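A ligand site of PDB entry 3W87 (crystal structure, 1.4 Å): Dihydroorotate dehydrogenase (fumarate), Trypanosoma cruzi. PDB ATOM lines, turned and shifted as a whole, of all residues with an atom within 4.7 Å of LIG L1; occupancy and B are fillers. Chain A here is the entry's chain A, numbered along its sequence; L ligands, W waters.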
ATOM      1  N   ALA A  20       3.014 -17.447 -21.175  1.00  0.00           N
ATOM      2  CA  ALA A  20       1.645 -17.603 -20.656  1.00  0.00           C
ATOM      3  C   ALA A  20       1.069 -18.940 -21.157  1.00  0.00           C
ATOM      4  O   ALA A  20       1.370 -19.392 -22.276  1.00  0.00           O
ATOM      5  CB  ALA A  20       0.773 -16.477 -21.244  1.00  0.00           C
ATOM      6  N   ALA A  21       0.304 -19.623 -20.303  1.00  0.00           N
ATOM      7  CA  ALA A  21      -0.276 -20.907 -20.723  1.00  0.00           C
ATOM      8  C   ALA A  21      -1.011 -20.777 -22.032  1.00  0.00           C
ATOM      9  O   ALA A  21      -1.687 -19.795 -22.339  1.00  0.00           O
ATOM     10  CB  ALA A  21      -1.215 -21.453 -19.631  1.00  0.00           C
ATOM     11  N   GLY A  22      -0.818 -21.815 -22.867  1.00  0.00           N
ATOM     12  CA  GLY A  22      -1.366 -21.849 -24.201  1.00  0.00           C
ATOM     13  C   GLY A  22      -0.511 -21.358 -25.320  1.00  0.00           C
ATOM     14  O   GLY A  22      -0.711 -21.709 -26.487  1.00  0.00           O
ATOM     15  N   VAL A  23       0.496 -20.524 -25.015  1.00  0.00           N
ATOM     16  CA  VAL A  23       1.401 -20.013 -26.040  1.00  0.00           C
ATOM     17  C   VAL A  23       2.738 -20.735 -26.029  1.00  0.00           C
ATOM     18  O   VAL A  23       3.354 -20.875 -24.970  1.00  0.00           O
ATOM     19  CB  VAL A  23       1.616 -18.503 -25.883  1.00  0.00           C
ATOM     20  CG1 VAL A  23       2.629 -17.996 -26.900  1.00  0.00           C
ATOM     21  CG2 VAL A  23       0.244 -17.792 -25.984  1.00  0.00           C
ATOM     22  N   LYS A  45       0.465 -26.074 -22.046  1.00  0.00           N
ATOM     23  CA  LYS A  45      -0.912 -25.735 -22.507  1.00  0.00           C
ATOM     24  C   LYS A  45      -1.892 -26.338 -21.526  1.00  0.00           C
ATOM     25  O   LYS A  45      -1.732 -27.501 -21.070  1.00  0.00           O
ATOM     26  CB  LYS A  45      -1.122 -26.461 -23.852  1.00  0.00           C
ATOM     27  CG  LYS A  45      -2.567 -26.447 -24.372  1.00  0.00           C
ATOM     28  CD  LYS A  45      -3.057 -25.067 -24.688  1.00  0.00           C
ATOM     29  CE  LYS A  45      -4.581 -25.032 -24.941  1.00  0.00           C
ATOM     30  NZ  LYS A  45      -5.036 -23.588 -25.209  1.00  0.00           N
ATOM     31  N   SER A  46      -2.914 -25.623 -21.169  1.00  0.00           N
ATOM     32  CA  SER A  46      -3.949 -26.251 -20.276  1.00  0.00           C
ATOM     33  C   SER A  46      -4.491 -27.551 -20.937  1.00  0.00           C
ATOM     34  O   SER A  46      -4.799 -27.616 -22.134  1.00  0.00           O
ATOM     35  CB  SER A  46      -5.180 -25.353 -20.137  1.00  0.00           C
ATOM     36  OG  SER A  46      -4.799 -24.174 -19.374  1.00  0.00           O
ATOM     37  N   TYR A  60      -7.288 -18.011 -33.942  1.00  0.00           N
ATOM     38  CA  TYR A  60      -6.424 -16.988 -33.314  1.00  0.00           C
ATOM     39  C   TYR A  60      -6.105 -16.017 -34.328  1.00  0.00           C
ATOM     40  O   TYR A  60      -5.761 -16.397 -35.480  1.00  0.00           O
ATOM     41  CB  TYR A  60      -5.141 -17.661 -32.882  1.00  0.00           C
ATOM     42  CG  TYR A  60      -4.076 -16.667 -32.421  1.00  0.00           C
ATOM     43  CD1 TYR A  60      -4.045 -16.153 -31.105  1.00  0.00           C
ATOM     44  CD2 TYR A  60      -3.127 -16.224 -33.310  1.00  0.00           C
ATOM     45  CE1 TYR A  60      -3.072 -15.150 -30.729  1.00  0.00           C
ATOM     46  CE2 TYR A  60      -2.128 -15.289 -32.925  1.00  0.00           C
ATOM     47  CZ  TYR A  60      -2.131 -14.754 -31.658  1.00  0.00           C
ATOM     48  OH  TYR A  60      -1.158 -13.869 -31.286  1.00  0.00           O
ATOM     49  N   SER A  67      -4.483  -9.515 -29.550  1.00  0.00           N
ATOM     50  CA  SER A  67      -4.936 -10.748 -30.202  1.00  0.00           C
ATOM     51  C   SER A  67      -6.321 -11.100 -29.695  1.00  0.00           C
ATOM     52  O   SER A  67      -6.811 -10.626 -28.683  1.00  0.00           O
ATOM     53  CB  SER A  67      -4.005 -11.941 -29.901  1.00  0.00           C
ATOM     54  OG  SER A  67      -4.066 -12.301 -28.518  1.00  0.00           O
ATOM     55  N   ASN A  69      -8.703 -14.827 -29.493  1.00  0.00           N
ATOM     56  CA  ASN A  69      -8.690 -16.310 -29.704  1.00  0.00           C
ATOM     57  C   ASN A  69      -9.898 -16.989 -29.127  1.00  0.00           C
ATOM     58  O   ASN A  69     -10.443 -16.637 -28.114  1.00  0.00           O
ATOM     59  CB  ASN A  69      -7.432 -16.979 -29.137  1.00  0.00           C
ATOM     60  CG  ASN A  69      -7.565 -17.392 -27.643  1.00  0.00           C
ATOM     61  OD1 ASN A  69      -8.067 -18.442 -27.273  1.00  0.00           O
ATOM     62  ND2 ASN A  69      -7.131 -16.507 -26.735  1.00  0.00           N
ATOM     63  N   MET A  71      -9.579 -20.801 -29.022  1.00  0.00           N
ATOM     64  CA  MET A  71      -8.876 -22.008 -29.426  1.00  0.00           C
ATOM     65  C   MET A  71      -9.758 -23.188 -29.192  1.00  0.00           C
ATOM     66  O   MET A  71      -9.622 -24.181 -30.006  1.00  0.00           O
ATOM     67  CB  MET A  71      -7.562 -22.153 -28.703  1.00  0.00           C
ATOM     68  CG  MET A  71      -6.541 -21.011 -28.826  1.00  0.00           C
ATOM     69  SD  MET A  71      -6.164 -20.595 -30.549  1.00  0.00           S
ATOM     70  CE  MET A  71      -5.101 -21.852 -30.947  1.00  0.00           C
ATOM     71  N   SER A  99      -0.395 -26.717 -16.533  1.00  0.00           N
ATOM     72  CA  SER A  99      -1.738 -26.106 -16.455  1.00  0.00           C
ATOM     73  C   SER A  99      -2.804 -27.176 -16.718  1.00  0.00           C
ATOM     74  O   SER A  99      -2.711 -27.944 -17.699  1.00  0.00           O
ATOM     75  CB  SER A  99      -1.860 -24.961 -17.499  1.00  0.00           C
ATOM     76  OG  SER A  99      -3.207 -24.472 -17.385  1.00  0.00           O
ATOM     77  N   GLU A 127      -0.609 -25.171 -12.158  1.00  0.00           N
ATOM     78  CA  GLU A 127      -1.422 -23.952 -12.388  1.00  0.00           C
ATOM     79  C   GLU A 127      -2.795 -24.422 -12.785  1.00  0.00           C
ATOM     80  O   GLU A 127      -3.003 -24.954 -13.849  1.00  0.00           O
ATOM     81  CB  GLU A 127      -0.734 -22.989 -13.420  1.00  0.00           C
ATOM     82  CG  GLU A 127      -1.600 -21.655 -13.589  1.00  0.00           C
ATOM     83  CD  GLU A 127      -0.932 -20.692 -14.532  1.00  0.00           C
ATOM     84  OE1 GLU A 127      -1.172 -20.830 -15.744  1.00  0.00           O
ATOM     85  OE2 GLU A 127      -0.149 -19.811 -14.053  1.00  0.00           O
ATOM     86  N   ASN A 129      -6.389 -23.868 -14.087  1.00  0.00           N
ATOM     87  CA  ASN A 129      -7.075 -22.830 -14.898  1.00  0.00           C
ATOM     88  C   ASN A 129      -8.543 -22.764 -14.542  1.00  0.00           C
ATOM     89  O   ASN A 129      -9.254 -23.679 -14.865  1.00  0.00           O
ATOM     90  CB  ASN A 129      -6.838 -23.158 -16.355  1.00  0.00           C
ATOM     91  CG  ASN A 129      -7.439 -22.177 -17.311  1.00  0.00           C
ATOM     92  OD1 ASN A 129      -8.061 -21.222 -16.910  1.00  0.00           O
ATOM     93  ND2 ASN A 129      -7.258 -22.413 -18.586  1.00  0.00           N
ATOM     94  N   LYS A 166      -5.069 -19.814 -12.140  1.00  0.00           N
ATOM     95  CA  LYS A 166      -5.120 -18.833 -13.245  1.00  0.00           C
ATOM     96  C   LYS A 166      -6.532 -18.239 -13.231  1.00  0.00           C
ATOM     97  O   LYS A 166      -7.537 -18.940 -13.411  1.00  0.00           O
ATOM     98  CB  LYS A 166      -4.842 -19.513 -14.578  1.00  0.00           C
ATOM     99  CG  LYS A 166      -4.901 -18.600 -15.832  1.00  0.00           C
ATOM    100  CD  LYS A 166      -3.727 -17.640 -15.884  1.00  0.00           C
ATOM    101  CE  LYS A 166      -3.662 -16.944 -17.278  1.00  0.00           C
ATOM    102  NZ  LYS A 166      -3.193 -17.850 -18.300  1.00  0.00           N
ATOM    103  N   VAL A 195      -3.651 -12.057 -15.520  1.00  0.00           N
ATOM    104  CA  VAL A 195      -5.000 -12.566 -15.826  1.00  0.00           C
ATOM    105  C   VAL A 195      -4.956 -13.450 -17.062  1.00  0.00           C
ATOM    106  O   VAL A 195      -4.043 -13.391 -17.925  1.00  0.00           O
ATOM    107  CB  VAL A 195      -5.978 -11.388 -16.105  1.00  0.00           C
ATOM    108  CG1 VAL A 195      -6.167 -10.538 -14.770  1.00  0.00           C
ATOM    109  CG2 VAL A 195      -5.484 -10.451 -17.190  1.00  0.00           C
ATOM    110  N   ASN A 196      -6.035 -14.229 -17.165  1.00  0.00           N
ATOM    111  CA  ASN A 196      -6.421 -14.837 -18.475  1.00  0.00           C
ATOM    112  C   ASN A 196      -6.943 -13.735 -19.410  1.00  0.00           C
ATOM    113  O   ASN A 196      -7.026 -12.551 -19.085  1.00  0.00           O
ATOM    114  CB  ASN A 196      -7.480 -15.951 -18.181  1.00  0.00           C
ATOM    115  CG  ASN A 196      -7.344 -17.116 -19.131  1.00  0.00           C
ATOM    116  OD1 ASN A 196      -7.258 -16.933 -20.346  1.00  0.00           O
ATOM    117  ND2 ASN A 196      -7.385 -18.297 -18.618  1.00  0.00           N
ATOM    118  N   SER A 197      -7.283 -14.171 -20.616  1.00  0.00           N
ATOM    119  CA  SER A 197      -7.759 -13.197 -21.611  1.00  0.00           C
ATOM    120  C   SER A 197      -9.011 -12.514 -21.142  1.00  0.00           C
ATOM    121  O   SER A 197      -9.816 -12.992 -20.340  1.00  0.00           O
ATOM    122  CB  SER A 197      -7.923 -13.909 -22.978  1.00  0.00           C
ATOM    123  OG  SER A 197      -8.649 -15.046 -22.890  1.00  0.00           O
ATOM    124  N   GLY A 223      -6.139 -10.582 -25.761  1.00  0.00           N
ATOM    125  CA  GLY A 223      -4.857 -10.369 -25.133  1.00  0.00           C
ATOM    126  C   GLY A 223      -4.071  -9.264 -25.717  1.00  0.00           C
ATOM    127  O   GLY A 223      -4.486  -8.684 -26.740  1.00  0.00           O
ATOM    128  N   GLY A 224      -2.901  -8.912 -25.134  1.00  0.00           N
ATOM    129  CA  GLY A 224      -2.020  -7.932 -25.712  1.00  0.00           C
ATOM    130  C   GLY A 224      -2.201  -6.515 -25.180  1.00  0.00           C
ATOM    131  O   GLY A 224      -2.658  -6.324 -24.004  1.00  0.00           O
ATOM    132  N   ILE A 227      -5.138  -5.062 -23.021  1.00  0.00           N
ATOM    133  CA  ILE A 227      -5.517  -5.497 -21.692  1.00  0.00           C
ATOM    134  C   ILE A 227      -4.549  -5.155 -20.623  1.00  0.00           C
ATOM    135  O   ILE A 227      -4.758  -5.503 -19.471  1.00  0.00           O
ATOM    136  CB  ILE A 227      -5.799  -7.051 -21.646  1.00  0.00           C
ATOM    137  CG1 ILE A 227      -4.552  -7.935 -21.665  1.00  0.00           C
ATOM    138  CG2 ILE A 227      -6.760  -7.471 -22.778  1.00  0.00           C
ATOM    139  CD1 ILE A 227      -4.860  -9.352 -21.220  1.00  0.00           C
ATOM    140  N   CYS A 250       0.136 -11.492 -15.785  1.00  0.00           N
ATOM    141  CA  CYS A 250       0.032 -11.880 -17.196  1.00  0.00           C
ATOM    142  C   CYS A 250      -0.907 -10.891 -17.852  1.00  0.00           C
ATOM    143  O   CYS A 250      -2.004 -10.634 -17.309  1.00  0.00           O
ATOM    144  CB  CYS A 250      -0.622 -13.296 -17.249  1.00  0.00           C
ATOM    145  SG  CYS A 250      -0.587 -13.980 -18.934  1.00  0.00           S
ATOM    146  N   GLY A 251      -0.519 -10.354 -18.992  1.00  0.00           N
ATOM    147  CA  GLY A 251      -1.442  -9.520 -19.758  1.00  0.00           C
ATOM    148  C   GLY A 251      -0.714  -8.329 -20.292  1.00  0.00           C
ATOM    149  O   GLY A 251      -0.237  -7.471 -19.486  1.00  0.00           O
ATOM    150  N   GLY A 252      -0.588  -8.218 -21.596  1.00  0.00           N
ATOM    151  CA  GLY A 252      -0.071  -6.971 -22.143  1.00  0.00           C
ATOM    152  C   GLY A 252       1.395  -6.734 -22.022  1.00  0.00           C
ATOM    153  O   GLY A 252       1.873  -5.611 -22.286  1.00  0.00           O
ATOM    154  N   VAL A 253       2.176  -7.771 -21.775  1.00  0.00           N
ATOM    155  CA  VAL A 253       3.670  -7.532 -21.657  1.00  0.00           C
ATOM    156  C   VAL A 253       4.319  -7.680 -23.052  1.00  0.00           C
ATOM    157  O   VAL A 253       4.292  -8.755 -23.660  1.00  0.00           O
ATOM    158  CB  VAL A 253       4.303  -8.601 -20.731  1.00  0.00           C
ATOM    159  CG1 VAL A 253       5.817  -8.403 -20.748  1.00  0.00           C
ATOM    160  CG2 VAL A 253       3.752  -8.381 -19.299  1.00  0.00           C
ATOM    161  N   GLN A 271       4.314 -13.367 -17.030  1.00  0.00           N
ATOM    162  CA  GLN A 271       4.022 -14.294 -18.157  1.00  0.00           C
ATOM    163  C   GLN A 271       3.749 -13.497 -19.421  1.00  0.00           C
ATOM    164  O   GLN A 271       3.251 -12.377 -19.362  1.00  0.00           O
ATOM    165  CB  GLN A 271       2.810 -15.160 -17.872  1.00  0.00           C
ATOM    166  CG  GLN A 271       2.871 -15.782 -16.443  1.00  0.00           C
ATOM    167  CD  GLN A 271       1.749 -16.795 -16.314  1.00  0.00           C
ATOM    168  OE1 GLN A 271       0.683 -16.752 -16.957  1.00  0.00           O
ATOM    169  NE2 GLN A 271       2.004 -17.817 -15.445  1.00  0.00           N
ATOM    170  N   VAL A 272       4.116 -14.100 -20.566  1.00  0.00           N
ATOM    171  CA  VAL A 272       4.071 -13.370 -21.888  1.00  0.00           C
ATOM    172  C   VAL A 272       3.310 -14.295 -22.815  1.00  0.00           C
ATOM    173  O   VAL A 272       3.733 -15.414 -23.105  1.00  0.00           O
ATOM    174  CB  VAL A 272       5.503 -13.141 -22.356  1.00  0.00           C
ATOM    175  CG1 VAL A 272       5.409 -12.242 -23.607  1.00  0.00           C
ATOM    176  CG2 VAL A 272       6.373 -12.465 -21.243  1.00  0.00           C
ATOM    177  N   GLY A 273       2.161 -13.793 -23.314  1.00  0.00           N
ATOM    178  CA  GLY A 273       1.295 -14.561 -24.188  1.00  0.00           C
ATOM    179  C   GLY A 273       1.377 -14.056 -25.622  1.00  0.00           C
ATOM    180  O   GLY A 273       2.250 -14.445 -26.399  1.00  0.00           O
ATOM    181  N   THR A 274       0.493 -13.077 -25.964  1.00  0.00           N
ATOM    182  CA  THR A 274       0.371 -12.516 -27.323  1.00  0.00           C
ATOM    183  C   THR A 274       1.759 -12.135 -27.853  1.00  0.00           C
ATOM    184  O   THR A 274       2.112 -12.448 -29.013  1.00  0.00           O
ATOM    185  CB  THR A 274      -0.572 -11.317 -27.333  1.00  0.00           C
ATOM    186  OG1 THR A 274      -1.865 -11.808 -26.943  1.00  0.00           O
ATOM    187  CG2 THR A 274      -0.642 -10.704 -28.715  1.00  0.00           C
HETATM  188  N1  LIG L   1      -4.652 -19.327 -20.743  1.00  0.00           N
HETATM  189  C1  LIG L   1      -4.662 -20.495 -20.019  1.00  0.00           C
HETATM  190  O1  LIG L   1      -4.625 -20.408 -18.806  1.00  0.00           O
HETATM  191  N2  LIG L   1      -4.605 -21.717 -20.677  1.00  0.00           N
HETATM  192  C2  LIG L   1      -4.522 -21.805 -21.992  1.00  0.00           C
HETATM  193  O2  LIG L   1      -4.432 -22.986 -22.480  1.00  0.00           O
HETATM  194  C3  LIG L   1      -4.566 -20.677 -22.799  1.00  0.00           C
HETATM  195  N3  LIG L   1      -4.460 -20.784 -24.103  1.00  0.00           N
HETATM  196  C4  LIG L   1      -4.214 -19.636 -24.830  1.00  0.00           C
HETATM  197  C5  LIG L   1      -4.044 -19.698 -26.181  1.00  0.00           C
HETATM  198  C6  LIG L   1      -3.743 -18.587 -26.957  1.00  0.00           C
HETATM  199  C7  LIG L   1      -3.531 -18.631 -28.474  1.00  0.00           C
HETATM  200  C8  LIG L   1      -3.764 -17.323 -26.343  1.00  0.00           C
HETATM  201  C9  LIG L   1      -3.463 -16.044 -27.064  1.00  0.00           C
HETATM  202  C10 LIG L   1      -3.965 -17.214 -24.972  1.00  0.00           C
HETATM  203  C11 LIG L   1      -4.214 -18.366 -24.205  1.00  0.00           C
HETATM  204  N4  LIG L   1      -4.447 -18.304 -22.837  1.00  0.00           N
HETATM  205  C12 LIG L   1      -4.527 -19.428 -22.073  1.00  0.00           C
HETATM  206  C13 LIG L   1      -4.408 -16.978 -22.136  1.00  0.00           C
HETATM  207  C14 LIG L   1      -3.001 -16.502 -21.921  1.00  0.00           C
HETATM  208  O3  LIG L   1      -2.331 -17.409 -21.018  1.00  0.00           O
HETATM  209  C15 LIG L   1      -2.962 -15.147 -21.278  1.00  0.00           C
HETATM  210  O4  LIG L   1      -3.634 -15.223 -20.000  1.00  0.00           O
HETATM  211  C16 LIG L   1      -3.639 -14.076 -22.136  1.00  0.00           C
HETATM  212  O5  LIG L   1      -3.335 -14.268 -23.526  1.00  0.00           O
HETATM  213  C17 LIG L   1      -3.217 -12.660 -21.716  1.00  0.00           C
HETATM  214  O6  LIG L   1      -1.818 -12.450 -21.822  1.00  0.00           O
HETATM  215  P1  LIG L   1      -1.196 -11.608 -23.067  1.00  0.00           P
HETATM  216  O7  LIG L   1       0.264 -11.694 -22.848  1.00  0.00           O
HETATM  217  O8  LIG L   1      -1.820 -10.247 -23.042  1.00  0.00           O
HETATM  218  O9  LIG L   1      -1.628 -12.341 -24.336  1.00  0.00           O
HETATM  219  O1  LG2 L   2      -7.867 -22.867 -25.313  1.00  0.00           O
HETATM  220  C1  LG2 L   2      -8.457 -21.730 -25.317  1.00  0.00           C
HETATM  221  O2  LG2 L   2      -9.355 -21.315 -26.037  1.00  0.00           O
HETATM  222  C2  LG2 L   2      -8.089 -20.830 -24.166  1.00  0.00           C
HETATM  223  N1  LG2 L   2      -7.955 -19.515 -24.556  1.00  0.00           N
HETATM  224  C3  LG2 L   2      -7.684 -18.571 -23.595  1.00  0.00           C
HETATM  225  O3  LG2 L   2      -7.542 -17.353 -23.966  1.00  0.00           O
HETATM  226  N2  LG2 L   2      -7.613 -18.874 -22.293  1.00  0.00           N
HETATM  227  C4  LG2 L   2      -7.756 -20.189 -21.833  1.00  0.00           C
HETATM  228  O4  LG2 L   2      -7.698 -20.370 -20.601  1.00  0.00           O
HETATM  229  C5  LG2 L   2      -7.996 -21.205 -22.830  1.00  0.00           C
HETATM  230  C6  LG2 L   2      -8.176 -22.649 -22.325  1.00  0.00           C
HETATM  231  C7  LG2 L   2      -9.604 -22.824 -21.673  1.00  0.00           C
HETATM  232  C8  LG2 L   2     -10.902 -22.457 -22.367  1.00  0.00           C
HETATM  233  C9  LG2 L   2     -11.891 -23.472 -22.092  1.00  0.00           C
HETATM  234  C10 LG2 L   2     -12.776 -23.662 -23.239  1.00  0.00           C
HETATM  235  C11 LG2 L   2     -13.213 -24.941 -23.295  1.00  0.00           C
HETATM  236  C12 LG2 L   2     -13.082 -22.672 -24.150  1.00  0.00           C
HETATM  237  C13 LG2 L   2     -13.966 -22.968 -25.197  1.00  0.00           C
HETATM  238  C14 LG2 L   2     -14.435 -24.302 -25.261  1.00  0.00           C
HETATM  239  C15 LG2 L   2     -14.070 -25.246 -24.292  1.00  0.00           C
HETATM  240  C16 LG2 L   2     -14.556 -26.552 -24.274  1.00  0.00           C
HETATM  241  C17 LG2 L   2     -15.498 -26.872 -25.270  1.00  0.00           C
HETATM  242  C18 LG2 L   2     -15.858 -25.940 -26.274  1.00  0.00           C
HETATM  243  C19 LG2 L   2     -15.352 -24.657 -26.242  1.00  0.00           C
HETATM  244  C20 LG2 L   2     -15.788 -23.772 -27.337  1.00  0.00           C
HETATM  245  O5  LG2 L   2     -15.181 -22.738 -27.662  1.00  0.00           O
HETATM  246  O6  LG2 L   2     -16.881 -24.251 -28.139  1.00  0.00           O
HETATM  247  C21 LG2 L   2     -17.294 -23.352 -29.219  1.00  0.00           C
HETATM  248  O   HOH W   1       1.878 -10.211 -24.566  1.00  0.00           O
HETATM  249  O   HOH W   2      -3.478 -21.980 -16.722  1.00  0.00           O
HETATM  250  O   HOH W   3       1.631 -10.595 -20.809  1.00  0.00           O
HETATM  251  O   HOH W   4      -5.635 -13.902 -24.815  1.00  0.00           O
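OD1 of Asn 196 sits at hydrogen-bond distance from N2 of LG2 L2 (2.8 Å). N of Gly 252 lies within hydrogen-bond range of O8 of LIG L1 (2.8 Å). An oxygen (O2) of LIG L1 sits at hydrogen-bond distance from the side-chain amino group of Lys 45 (2.9 Å). A nitrogen (N2) of LIG L1 is in hydrogen-bond range of the side-chain hydroxyl of Ser 46, 2.8 Å away. The side-chain hydroxyl (OG) of Ser 197 sits at hydrogen-bond distance from an oxygen (O3) of LG2 L2. O7 of LIG L1 sits at hydrogen-bond distance from N of Gly 273 (2.9 Å). An oxygen (O9) of LIG L1 is in hydrogen-bond range of the side-chain hydroxyl of Thr 274. The side-chain amide nitrogen of Asn 196 sits at hydrogen-bond distance from an oxygen (O1) of LIG L1 (3.5 Å). O4 of LIG L1 is in hydrogen-bond range of SG of Cys 250 (3.5 Å). An oxygen (O3) of LIG L1 is in hydrogen-bond range of the backbone carbonyl oxygen (O) of Ala 21, 2.8 Å away. The backbone NH (N) of Ser 46 is in hydrogen-bond range of an oxygen (O2) of LIG L1 (3.3 Å). The side-chain amide nitrogen (ND2) of Asn 129 sits at hydrogen-bond distance from an oxygen (O4) of LG2 L2. N of Gly 224 is in hydrogen-bond range of O8 of LIG L1, 2.7 Å away. A nitrogen (N1) of LG2 L2 lies within hydrogen-bond range of the side-chain amide oxygen (OD1) of Asn 69 (2.9 Å). An oxygen (O2) of LG2 L2 lies within hydrogen-bond range of the backbone NH of Met 71, at 3.0 Å. The backbone NH (N) of Thr 274 sits at hydrogen-bond distance from an oxygen (O9) of LIG L1 (2.8 Å). The side-chain amino group (NZ) of Lys 45 is in salt-bridge range of an oxygen (O1) of LG2 L2. O1 of LIG L1 is in hydrogen-bond range of ND2 of Asn 129 (3.3 Å). O of Val 195 is in hydrogen-bond range of O4 of LIG L1 (2.8 Å). The side-chain amino group (NZ) of Lys 166 sits at hydrogen-bond distance from an oxygen (O3) of LIG L1 (2.9 Å).
A nitrogen (N2) of LG2 L2 lies close to a nitrogen (N1) of LIG L1 (3.4 Å).
OG of Ser 99 lies within hydrogen-bond range of OG of Ser 46 (2.6 Å). SG of Cys 250 is in hydrogen-bond range of OE1 of Gln 271 (3.6 Å). OD1 of Asn 69 is in hydrogen-bond range of N of Met 71. The side-chain amide nitrogen (ND2) of Asn 129 is in hydrogen-bond range of the side-chain hydroxyl (OG) of Ser 46, at 3.1 Å. The backbone carbonyl oxygen (O) of Gly 223 is in hydrogen-bond range of the backbone NH (N) of Ser 67 (2.9 Å). N of Ala 20 sits at hydrogen-bond distance from O of Val 272 (2.9 Å). The side-chain hydroxyl (OG) of Ser 67 lies within hydrogen-bond range of the side-chain hydroxyl (OG1) of Thr 274 (2.8 Å). The side-chain hydroxyl of Ser 197 is in hydrogen-bond range of the side-chain amide oxygen of Asn 196 (3.5 Å).
Ala 20 touches LIG L1. Gly 22 touches LIG L1 (CA to N3, 3.3 Å). Tyr 60 touches LIG L1 (CD1 to C7, 3.7 Å). ND2 of Asn 69 touches C8 of LIG L1, 3.5 Å away. Met 71 touches LIG L1. Ser 197 touches LIG L1. C of Gly 223 touches O8 of LIG L1, at 3.6 Å. Ile 227 touches LIG L1. Gly 251 touches LIG L1 (CA to O8, 3.4 Å). The nearest printed residue that does not touch LIG L1 is Val 272 (4.01 Å).
Water W4 bridges an oxygen (O5) of LIG L1 (2.7 Å) and the backbone NH of Gly 223 (3.5 Å). Water W1 lies within hydrogen-bond range of an oxygen (O7) of LIG L1, the backbone carbonyl oxygen of Val 253 and the backbone NH of Thr 274. Water W2 lies within hydrogen-bond range of the side-chain hydroxyl (OG) of Ser 99 (2.6 Å), the side-chain carboxylate (OE1) of Glu 127 (2.8 Å) and an oxygen (O1) of LIG L1 (2.9 Å).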
